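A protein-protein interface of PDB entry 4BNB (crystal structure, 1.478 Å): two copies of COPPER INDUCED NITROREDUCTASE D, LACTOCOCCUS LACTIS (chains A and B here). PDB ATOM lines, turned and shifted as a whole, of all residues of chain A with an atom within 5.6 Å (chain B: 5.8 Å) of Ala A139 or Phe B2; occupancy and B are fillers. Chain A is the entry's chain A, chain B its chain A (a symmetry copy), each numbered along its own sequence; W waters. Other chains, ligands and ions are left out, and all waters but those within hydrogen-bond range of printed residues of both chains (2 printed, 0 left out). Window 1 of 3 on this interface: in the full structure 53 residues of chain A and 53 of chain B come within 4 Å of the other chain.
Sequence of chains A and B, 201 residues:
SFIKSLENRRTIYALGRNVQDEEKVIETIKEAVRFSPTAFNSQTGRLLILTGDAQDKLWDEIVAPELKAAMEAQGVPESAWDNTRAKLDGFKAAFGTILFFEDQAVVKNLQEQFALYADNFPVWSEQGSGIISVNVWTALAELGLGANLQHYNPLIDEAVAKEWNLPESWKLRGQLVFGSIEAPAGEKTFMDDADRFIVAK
Ala A139 touches just one residue of chain B: Phe B2. Of chain A, only Phe A2, Ser A5, Asn A135, Thr A138, Ala A139 and Glu A142 come within 4 Å of Phe B2. Of the printed residues of chain B, Thr A28 touches Ile B3. Of the printed residues of chain B, Glu A142 touches Ser B1 and Phe B2. Of the printed residues of chain B, Phe A2 touches Phe B2 (3.6 Å) and Ser B5 (3.8 Å). Of the printed residues of chain B, Ala A32 touches Ile B3 and Leu B6. The nearest residue of chain A that does not touch Phe B2 is Leu A6 (4.7 Å). The nearest printed residue of chain B that does not touch Thr A138 is Leu B6 (7.0 Å).
N of Lys B4 sits close to OG of Ser B1 (3.2 Å). The side-chain hydroxyl of Thr A138 sits at hydrogen-bond distance from the backbone carbonyl oxygen of Val A134. The backbone carbonyl oxygen of Ser B1 lies within hydrogen-bond range of the side-chain hydroxyl of Ser B5 (3.2 Å).
Phe B2 touches its own counterpart, Phe A2. Phe A2 touches Ser B5, and with the chains exchanged Ser A5 touches Phe B2. Of the 12 pairs that touch across the chains among the printed residues, 3 have their exchanged pair printed and touching as well.
Among the printed residues, merely in contact across the chains: Asn A135 with Phe B2 (3.3 Å), Thr A138 with Phe B2 (3.4 Å), Asn A135 with Leu B6 (3.5 Å), Ala A139 with Phe B2 (3.6 Å), Phe A2 with Phe B2 (3.6 Å), Glu A142 with Ser B1 (3.6 Å), Ser A5 with Phe B2 (3.8 Å), Phe A2 with Ser B5 (3.8 Å), Ala A32 with Ile B3 (3.8 Å), Ala A32 with Leu B6 (3.9 Å) and Thr A28 with Ile B3 (3.97 Å).
Hydrophobic or aromatic side chains of chain B that line the printed part of chain A: Phe B2, Ile B3 and Leu B6.
Water W1 lies within hydrogen-bond range of OE1 of Glu A142 (2.6 Å), OG of Ser B1 (2.8 Å), N of Ile B3 (3.0 Å) and N of Phe B2 (3.2 Å). Water W2 lies within hydrogen-bond range of OG of Ser A5 (3.1 Å) and OG of Ser B5 (3.1 Å).
N of Phe B2 lies within hydrogen-bond range of OE2 of Glu A142 (2.8 Å).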
ATOM      1  N   PHE A   2      15.857  -0.671 -10.324  1.00  0.00           N
ATOM      2  CA  PHE A   2      14.841  -0.772 -11.366  1.00  0.00           C
ATOM      3  C   PHE A   2      15.463  -0.826 -12.762  1.00  0.00           C
ATOM      4  O   PHE A   2      15.049  -1.620 -13.606  1.00  0.00           O
ATOM      5  CB  PHE A   2      13.857   0.395 -11.272  1.00  0.00           C
ATOM      6  CG  PHE A   2      12.827   0.403 -12.363  1.00  0.00           C
ATOM      7  CD1 PHE A   2      11.786  -0.510 -12.355  1.00  0.00           C
ATOM      8  CD2 PHE A   2      12.902   1.319 -13.401  1.00  0.00           C
ATOM      9  CE1 PHE A   2      10.842  -0.510 -13.361  1.00  0.00           C
ATOM     10  CE2 PHE A   2      11.958   1.322 -14.411  1.00  0.00           C
ATOM     11  CZ  PHE A   2      10.927   0.406 -14.390  1.00  0.00           C
ATOM     12  N   SER A   5      16.706  -4.150 -13.407  1.00  0.00           N
ATOM     13  CA  SER A   5      15.595  -5.050 -13.701  1.00  0.00           C
ATOM     14  C   SER A   5      15.211  -4.947 -15.172  1.00  0.00           C
ATOM     15  O   SER A   5      14.969  -5.956 -15.833  1.00  0.00           O
ATOM     16  CB  SER A   5      14.381  -4.733 -12.820  1.00  0.00           C
ATOM     17  OG  SER A   5      14.655  -4.994 -11.452  1.00  0.00           O
ATOM     18  N   LEU A   6      15.164  -3.724 -15.689  1.00  0.00           N
ATOM     19  CA  LEU A   6      14.834  -3.514 -17.092  1.00  0.00           C
ATOM     20  C   LEU A   6      15.876  -4.163 -17.988  1.00  0.00           C
ATOM     21  O   LEU A   6      15.538  -4.835 -18.960  1.00  0.00           O
ATOM     22  CB  LEU A   6      14.741  -2.021 -17.418  1.00  0.00           C
ATOM     23  CG  LEU A   6      13.579  -1.221 -16.826  1.00  0.00           C
ATOM     24  CD1 LEU A   6      13.601   0.193 -17.389  1.00  0.00           C
ATOM     25  CD2 LEU A   6      12.233  -1.880 -17.098  1.00  0.00           C
ATOM     26  N   THR A  28       3.108 -13.383  -9.432  1.00  0.00           N
ATOM     27  CA  THR A  28       3.926 -12.291  -9.938  1.00  0.00           C
ATOM     28  C   THR A  28       3.333 -11.716 -11.224  1.00  0.00           C
ATOM     29  O   THR A  28       3.346 -10.503 -11.430  1.00  0.00           O
ATOM     30  CB  THR A  28       5.374 -12.758 -10.163  1.00  0.00           C
ATOM     31  OG1 THR A  28       5.904 -13.267  -8.934  1.00  0.00           O
ATOM     32  CG2 THR A  28       6.244 -11.612 -10.633  1.00  0.00           C
ATOM     33  N   ALA A  32       2.122  -7.787 -11.569  1.00  0.00           N
ATOM     34  CA  ALA A  32       2.690  -6.916 -12.591  1.00  0.00           C
ATOM     35  C   ALA A  32       1.584  -6.205 -13.361  1.00  0.00           C
ATOM     36  O   ALA A  32       1.693  -5.024 -13.672  1.00  0.00           O
ATOM     37  CB  ALA A  32       3.575  -7.712 -13.537  1.00  0.00           C
ATOM     38  N   VAL A 134       5.110  -5.856 -21.066  1.00  0.00           N
ATOM     39  CA  VAL A 134       6.509  -5.728 -20.665  1.00  0.00           C
ATOM     40  C   VAL A 134       6.686  -5.748 -19.152  1.00  0.00           C
ATOM     41  O   VAL A 134       7.712  -6.206 -18.664  1.00  0.00           O
ATOM     42  CB  VAL A 134       7.197  -4.471 -21.254  1.00  0.00           C
ATOM     43  CG1 VAL A 134       7.103  -4.487 -22.768  1.00  0.00           C
ATOM     44  CG2 VAL A 134       6.615  -3.185 -20.665  1.00  0.00           C
ATOM     45  N   ASN A 135       5.701  -5.261 -18.404  1.00  0.00           N
ATOM     46  CA  ASN A 135       5.791  -5.352 -16.953  1.00  0.00           C
ATOM     47  C   ASN A 135       5.768  -6.815 -16.500  1.00  0.00           C
ATOM     48  O   ASN A 135       6.534  -7.204 -15.624  1.00  0.00           O
ATOM     49  CB  ASN A 135       4.701  -4.527 -16.262  1.00  0.00           C
ATOM     50  CG  ASN A 135       5.054  -3.052 -16.185  1.00  0.00           C
ATOM     51  OD1 ASN A 135       6.216  -2.671 -16.338  1.00  0.00           O
ATOM     52  ND2 ASN A 135       4.055  -2.214 -15.943  1.00  0.00           N
ATOM     53  N   VAL A 136       4.914  -7.631 -17.111  1.00  0.00           N
ATOM     54  CA  VAL A 136       4.905  -9.062 -16.818  1.00  0.00           C
ATOM     55  C   VAL A 136       6.224  -9.708 -17.257  1.00  0.00           C
ATOM     56  O   VAL A 136       6.832 -10.484 -16.521  1.00  0.00           O
ATOM     57  CB  VAL A 136       3.724  -9.767 -17.512  1.00  0.00           C
ATOM     58  CG1 VAL A 136       3.874 -11.282 -17.430  1.00  0.00           C
ATOM     59  CG2 VAL A 136       2.405  -9.330 -16.887  1.00  0.00           C
ATOM     60  N   TRP A 137       6.659  -9.368 -18.463  1.00  0.00           N
ATOM     61  CA  TRP A 137       7.895  -9.884 -19.032  1.00  0.00           C
ATOM     62  C   TRP A 137       9.069  -9.614 -18.087  1.00  0.00           C
ATOM     63  O   TRP A 137       9.857 -10.511 -17.772  1.00  0.00           O
ATOM     64  CB  TRP A 137       8.101  -9.188 -20.372  1.00  0.00           C
ATOM     65  CG  TRP A 137       9.081  -9.784 -21.323  1.00  0.00           C
ATOM     66  CD1 TRP A 137      10.026 -10.731 -21.069  1.00  0.00           C
ATOM     67  CD2 TRP A 137       9.205  -9.451 -22.706  1.00  0.00           C
ATOM     68  NE1 TRP A 137      10.738 -11.007 -22.218  1.00  0.00           N
ATOM     69  CE2 TRP A 137      10.246 -10.232 -23.237  1.00  0.00           C
ATOM     70  CE3 TRP A 137       8.532  -8.562 -23.547  1.00  0.00           C
ATOM     71  CZ2 TRP A 137      10.631 -10.152 -24.572  1.00  0.00           C
ATOM     72  CZ3 TRP A 137       8.916  -8.481 -24.868  1.00  0.00           C
ATOM     73  CH2 TRP A 137       9.953  -9.273 -25.369  1.00  0.00           C
ATOM     74  N   THR A 138       9.169  -8.376 -17.616  1.00  0.00           N
ATOM     75  CA  THR A 138      10.268  -7.979 -16.746  1.00  0.00           C
ATOM     76  C   THR A 138      10.166  -8.650 -15.375  1.00  0.00           C
ATOM     77  O   THR A 138      11.176  -9.046 -14.793  1.00  0.00           O
ATOM     78  CB  THR A 138      10.323  -6.446 -16.593  1.00  0.00           C
ATOM     79  OG1 THR A 138      10.419  -5.843 -17.891  1.00  0.00           O
ATOM     80  CG2 THR A 138      11.526  -6.030 -15.771  1.00  0.00           C
ATOM     81  N   ALA A 139       8.949  -8.791 -14.864  1.00  0.00           N
ATOM     82  CA  ALA A 139       8.742  -9.454 -13.583  1.00  0.00           C
ATOM     83  C   ALA A 139       9.163 -10.923 -13.652  1.00  0.00           C
ATOM     84  O   ALA A 139       9.741 -11.458 -12.701  1.00  0.00           O
ATOM     85  CB  ALA A 139       7.286  -9.336 -13.153  1.00  0.00           C
ATOM     86  N   LEU A 140       8.875 -11.577 -14.776  1.00  0.00           N
ATOM     87  CA  LEU A 140       9.295 -12.961 -14.964  1.00  0.00           C
ATOM     88  C   LEU A 140      10.818 -13.064 -14.998  1.00  0.00           C
ATOM     89  O   LEU A 140      11.400 -13.980 -14.418  1.00  0.00           O
ATOM     90  CB  LEU A 140       8.701 -13.538 -16.249  1.00  0.00           C
ATOM     91  CG  LEU A 140       7.187 -13.749 -16.237  1.00  0.00           C
ATOM     92  CD1 LEU A 140       6.681 -14.058 -17.638  1.00  0.00           C
ATOM     93  CD2 LEU A 140       6.802 -14.860 -15.273  1.00  0.00           C
ATOM     94  N   ALA A 141      11.461 -12.117 -15.671  1.00  0.00           N
ATOM     95  CA  ALA A 141      12.915 -12.104 -15.748  1.00  0.00           C
ATOM     96  C   ALA A 141      13.539 -11.968 -14.361  1.00  0.00           C
ATOM     97  O   ALA A 141      14.589 -12.548 -14.089  1.00  0.00           O
ATOM     98  CB  ALA A 141      13.394 -10.989 -16.672  1.00  0.00           C
ATOM     99  N   GLU A 142      12.890 -11.217 -13.477  1.00  0.00           N
ATOM    100  CA  GLU A 142      13.399 -11.070 -12.118  1.00  0.00           C
ATOM    101  C   GLU A 142      13.393 -12.401 -11.370  1.00  0.00           C
ATOM    102  O   GLU A 142      14.242 -12.641 -10.509  1.00  0.00           O
ATOM    103  CB  GLU A 142      12.594 -10.039 -11.333  1.00  0.00           C
ATOM    104  CG  GLU A 142      13.115  -9.858  -9.917  1.00  0.00           C
ATOM    105  CD  GLU A 142      12.283  -8.899  -9.099  1.00  0.00           C
ATOM    106  OE1 GLU A 142      11.065  -9.136  -8.961  1.00  0.00           O
ATOM    107  OE2 GLU A 142      12.851  -7.909  -8.592  1.00  0.00           O
ATOM    108  N   LEU A 143      12.435 -13.262 -11.699  1.00  0.00           N
ATOM    109  CA  LEU A 143      12.370 -14.593 -11.101  1.00  0.00           C
ATOM    110  C   LEU A 143      13.380 -15.546 -11.736  1.00  0.00           C
ATOM    111  O   LEU A 143      13.483 -16.702 -11.331  1.00  0.00           O
ATOM    112  CB  LEU A 143      10.966 -15.182 -11.253  1.00  0.00           C
ATOM    113  CG  LEU A 143       9.817 -14.428 -10.581  1.00  0.00           C
ATOM    114  CD1 LEU A 143       8.510 -15.161 -10.831  1.00  0.00           C
ATOM    115  CD2 LEU A 143      10.071 -14.261  -9.093  1.00  0.00           C
ATOM    116  N   SER B   1      12.450  -4.807  -4.773  1.00  0.00           N
ATOM    117  CA  SER B   1      12.044  -5.765  -5.789  1.00  0.00           C
ATOM    118  C   SER B   1      11.347  -5.046  -6.944  1.00  0.00           C
ATOM    119  O   SER B   1      10.925  -3.896  -6.808  1.00  0.00           O
ATOM    120  CB  SER B   1      11.109  -6.817  -5.185  1.00  0.00           C
ATOM    121  OG  SER B   1       9.777  -6.336  -5.091  1.00  0.00           O
ATOM    122  N   PHE B   2      11.227  -5.725  -8.079  1.00  0.00           N
ATOM    123  CA  PHE B   2      10.621  -5.126  -9.264  1.00  0.00           C
ATOM    124  C   PHE B   2       9.141  -4.810  -9.047  1.00  0.00           C
ATOM    125  O   PHE B   2       8.662  -3.742  -9.429  1.00  0.00           O
ATOM    126  CB  PHE B   2      10.792  -6.044 -10.476  1.00  0.00           C
ATOM    127  CG  PHE B   2      10.123  -5.533 -11.717  1.00  0.00           C
ATOM    128  CD1 PHE B   2      10.660  -4.465 -12.417  1.00  0.00           C
ATOM    129  CD2 PHE B   2       8.953  -6.114 -12.183  1.00  0.00           C
ATOM    130  CE1 PHE B   2      10.043  -3.987 -13.554  1.00  0.00           C
ATOM    131  CE2 PHE B   2       8.333  -5.636 -13.323  1.00  0.00           C
ATOM    132  CZ  PHE B   2       8.879  -4.573 -14.009  1.00  0.00           C
ATOM    133  N   ILE B   3       8.410  -5.736  -8.440  1.00  0.00           N
ATOM    134  CA  ILE B   3       6.992  -5.505  -8.187  1.00  0.00           C
ATOM    135  C   ILE B   3       6.815  -4.292  -7.279  1.00  0.00           C
ATOM    136  O   ILE B   3       5.916  -3.481  -7.492  1.00  0.00           O
ATOM    137  CB  ILE B   3       6.306  -6.738  -7.575  1.00  0.00           C
ATOM    138  CG1 ILE B   3       6.273  -7.888  -8.588  1.00  0.00           C
ATOM    139  CG2 ILE B   3       4.891  -6.397  -7.127  1.00  0.00           C
ATOM    140  CD1 ILE B   3       5.531  -7.569  -9.879  1.00  0.00           C
ATOM    141  N   LYS B   4       7.679  -4.164  -6.276  1.00  0.00           N
ATOM    142  CA  LYS B   4       7.650  -3.004  -5.394  1.00  0.00           C
ATOM    143  C   LYS B   4       7.895  -1.716  -6.183  1.00  0.00           C
ATOM    144  O   LYS B   4       7.254  -0.690  -5.929  1.00  0.00           O
ATOM    145  CB  LYS B   4       8.687  -3.149  -4.278  1.00  0.00           C
ATOM    146  CG  LYS B   4       8.428  -4.317  -3.343  1.00  0.00           C
ATOM    147  CD  LYS B   4       7.110  -4.179  -2.605  1.00  0.00           C
ATOM    148  CE  LYS B   4       6.763  -5.462  -1.874  1.00  0.00           C
ATOM    149  NZ  LYS B   4       7.805  -5.835  -0.879  1.00  0.00           N
ATOM    150  N   SER B   5       8.821  -1.769  -7.135  1.00  0.00           N
ATOM    151  CA  SER B   5       9.101  -0.614  -7.983  1.00  0.00           C
ATOM    152  C   SER B   5       7.849  -0.217  -8.757  1.00  0.00           C
ATOM    153  O   SER B   5       7.527   0.966  -8.871  1.00  0.00           O
ATOM    154  CB  SER B   5      10.246  -0.910  -8.956  1.00  0.00           C
ATOM    155  OG  SER B   5      11.470  -1.108  -8.267  1.00  0.00           O
ATOM    156  N   LEU B   6       7.137  -1.206  -9.283  1.00  0.00           N
ATOM    157  CA  LEU B   6       5.909  -0.940 -10.019  1.00  0.00           C
ATOM    158  C   LEU B   6       4.874  -0.293  -9.114  1.00  0.00           C
ATOM    159  O   LEU B   6       4.228   0.681  -9.494  1.00  0.00           O
ATOM    160  CB  LEU B   6       5.332  -2.227 -10.613  1.00  0.00           C
ATOM    161  CG  LEU B   6       6.096  -2.906 -11.753  1.00  0.00           C
ATOM    162  CD1 LEU B   6       5.279  -4.076 -12.281  1.00  0.00           C
ATOM    163  CD2 LEU B   6       6.423  -1.934 -12.880  1.00  0.00           C
ATOM    164  N   GLU B   7       4.723  -0.829  -7.909  1.00  0.00           N
ATOM    165  CA  GLU B   7       3.720  -0.317  -6.984  1.00  0.00           C
ATOM    166  C   GLU B   7       4.035   1.117  -6.564  1.00  0.00           C
ATOM    167  O   GLU B   7       3.126   1.907  -6.303  1.00  0.00           O
ATOM    168  CB  GLU B   7       3.616  -1.212  -5.746  1.00  0.00           C
ATOM    169  CG  GLU B   7       2.470  -0.831  -4.825  1.00  0.00           C
ATOM    170  CD  GLU B   7       2.175  -1.885  -3.779  1.00  0.00           C
ATOM    171  OE1 GLU B   7       2.943  -2.867  -3.673  1.00  0.00           O
ATOM    172  OE2 GLU B   7       1.168  -1.727  -3.059  1.00  0.00           O
HETATM  173  O   HOH W   1       9.422  -8.217  -7.202  1.00  0.00           O
HETATM  174  O   HOH W   2      13.530  -3.194  -9.217  1.00  0.00           O
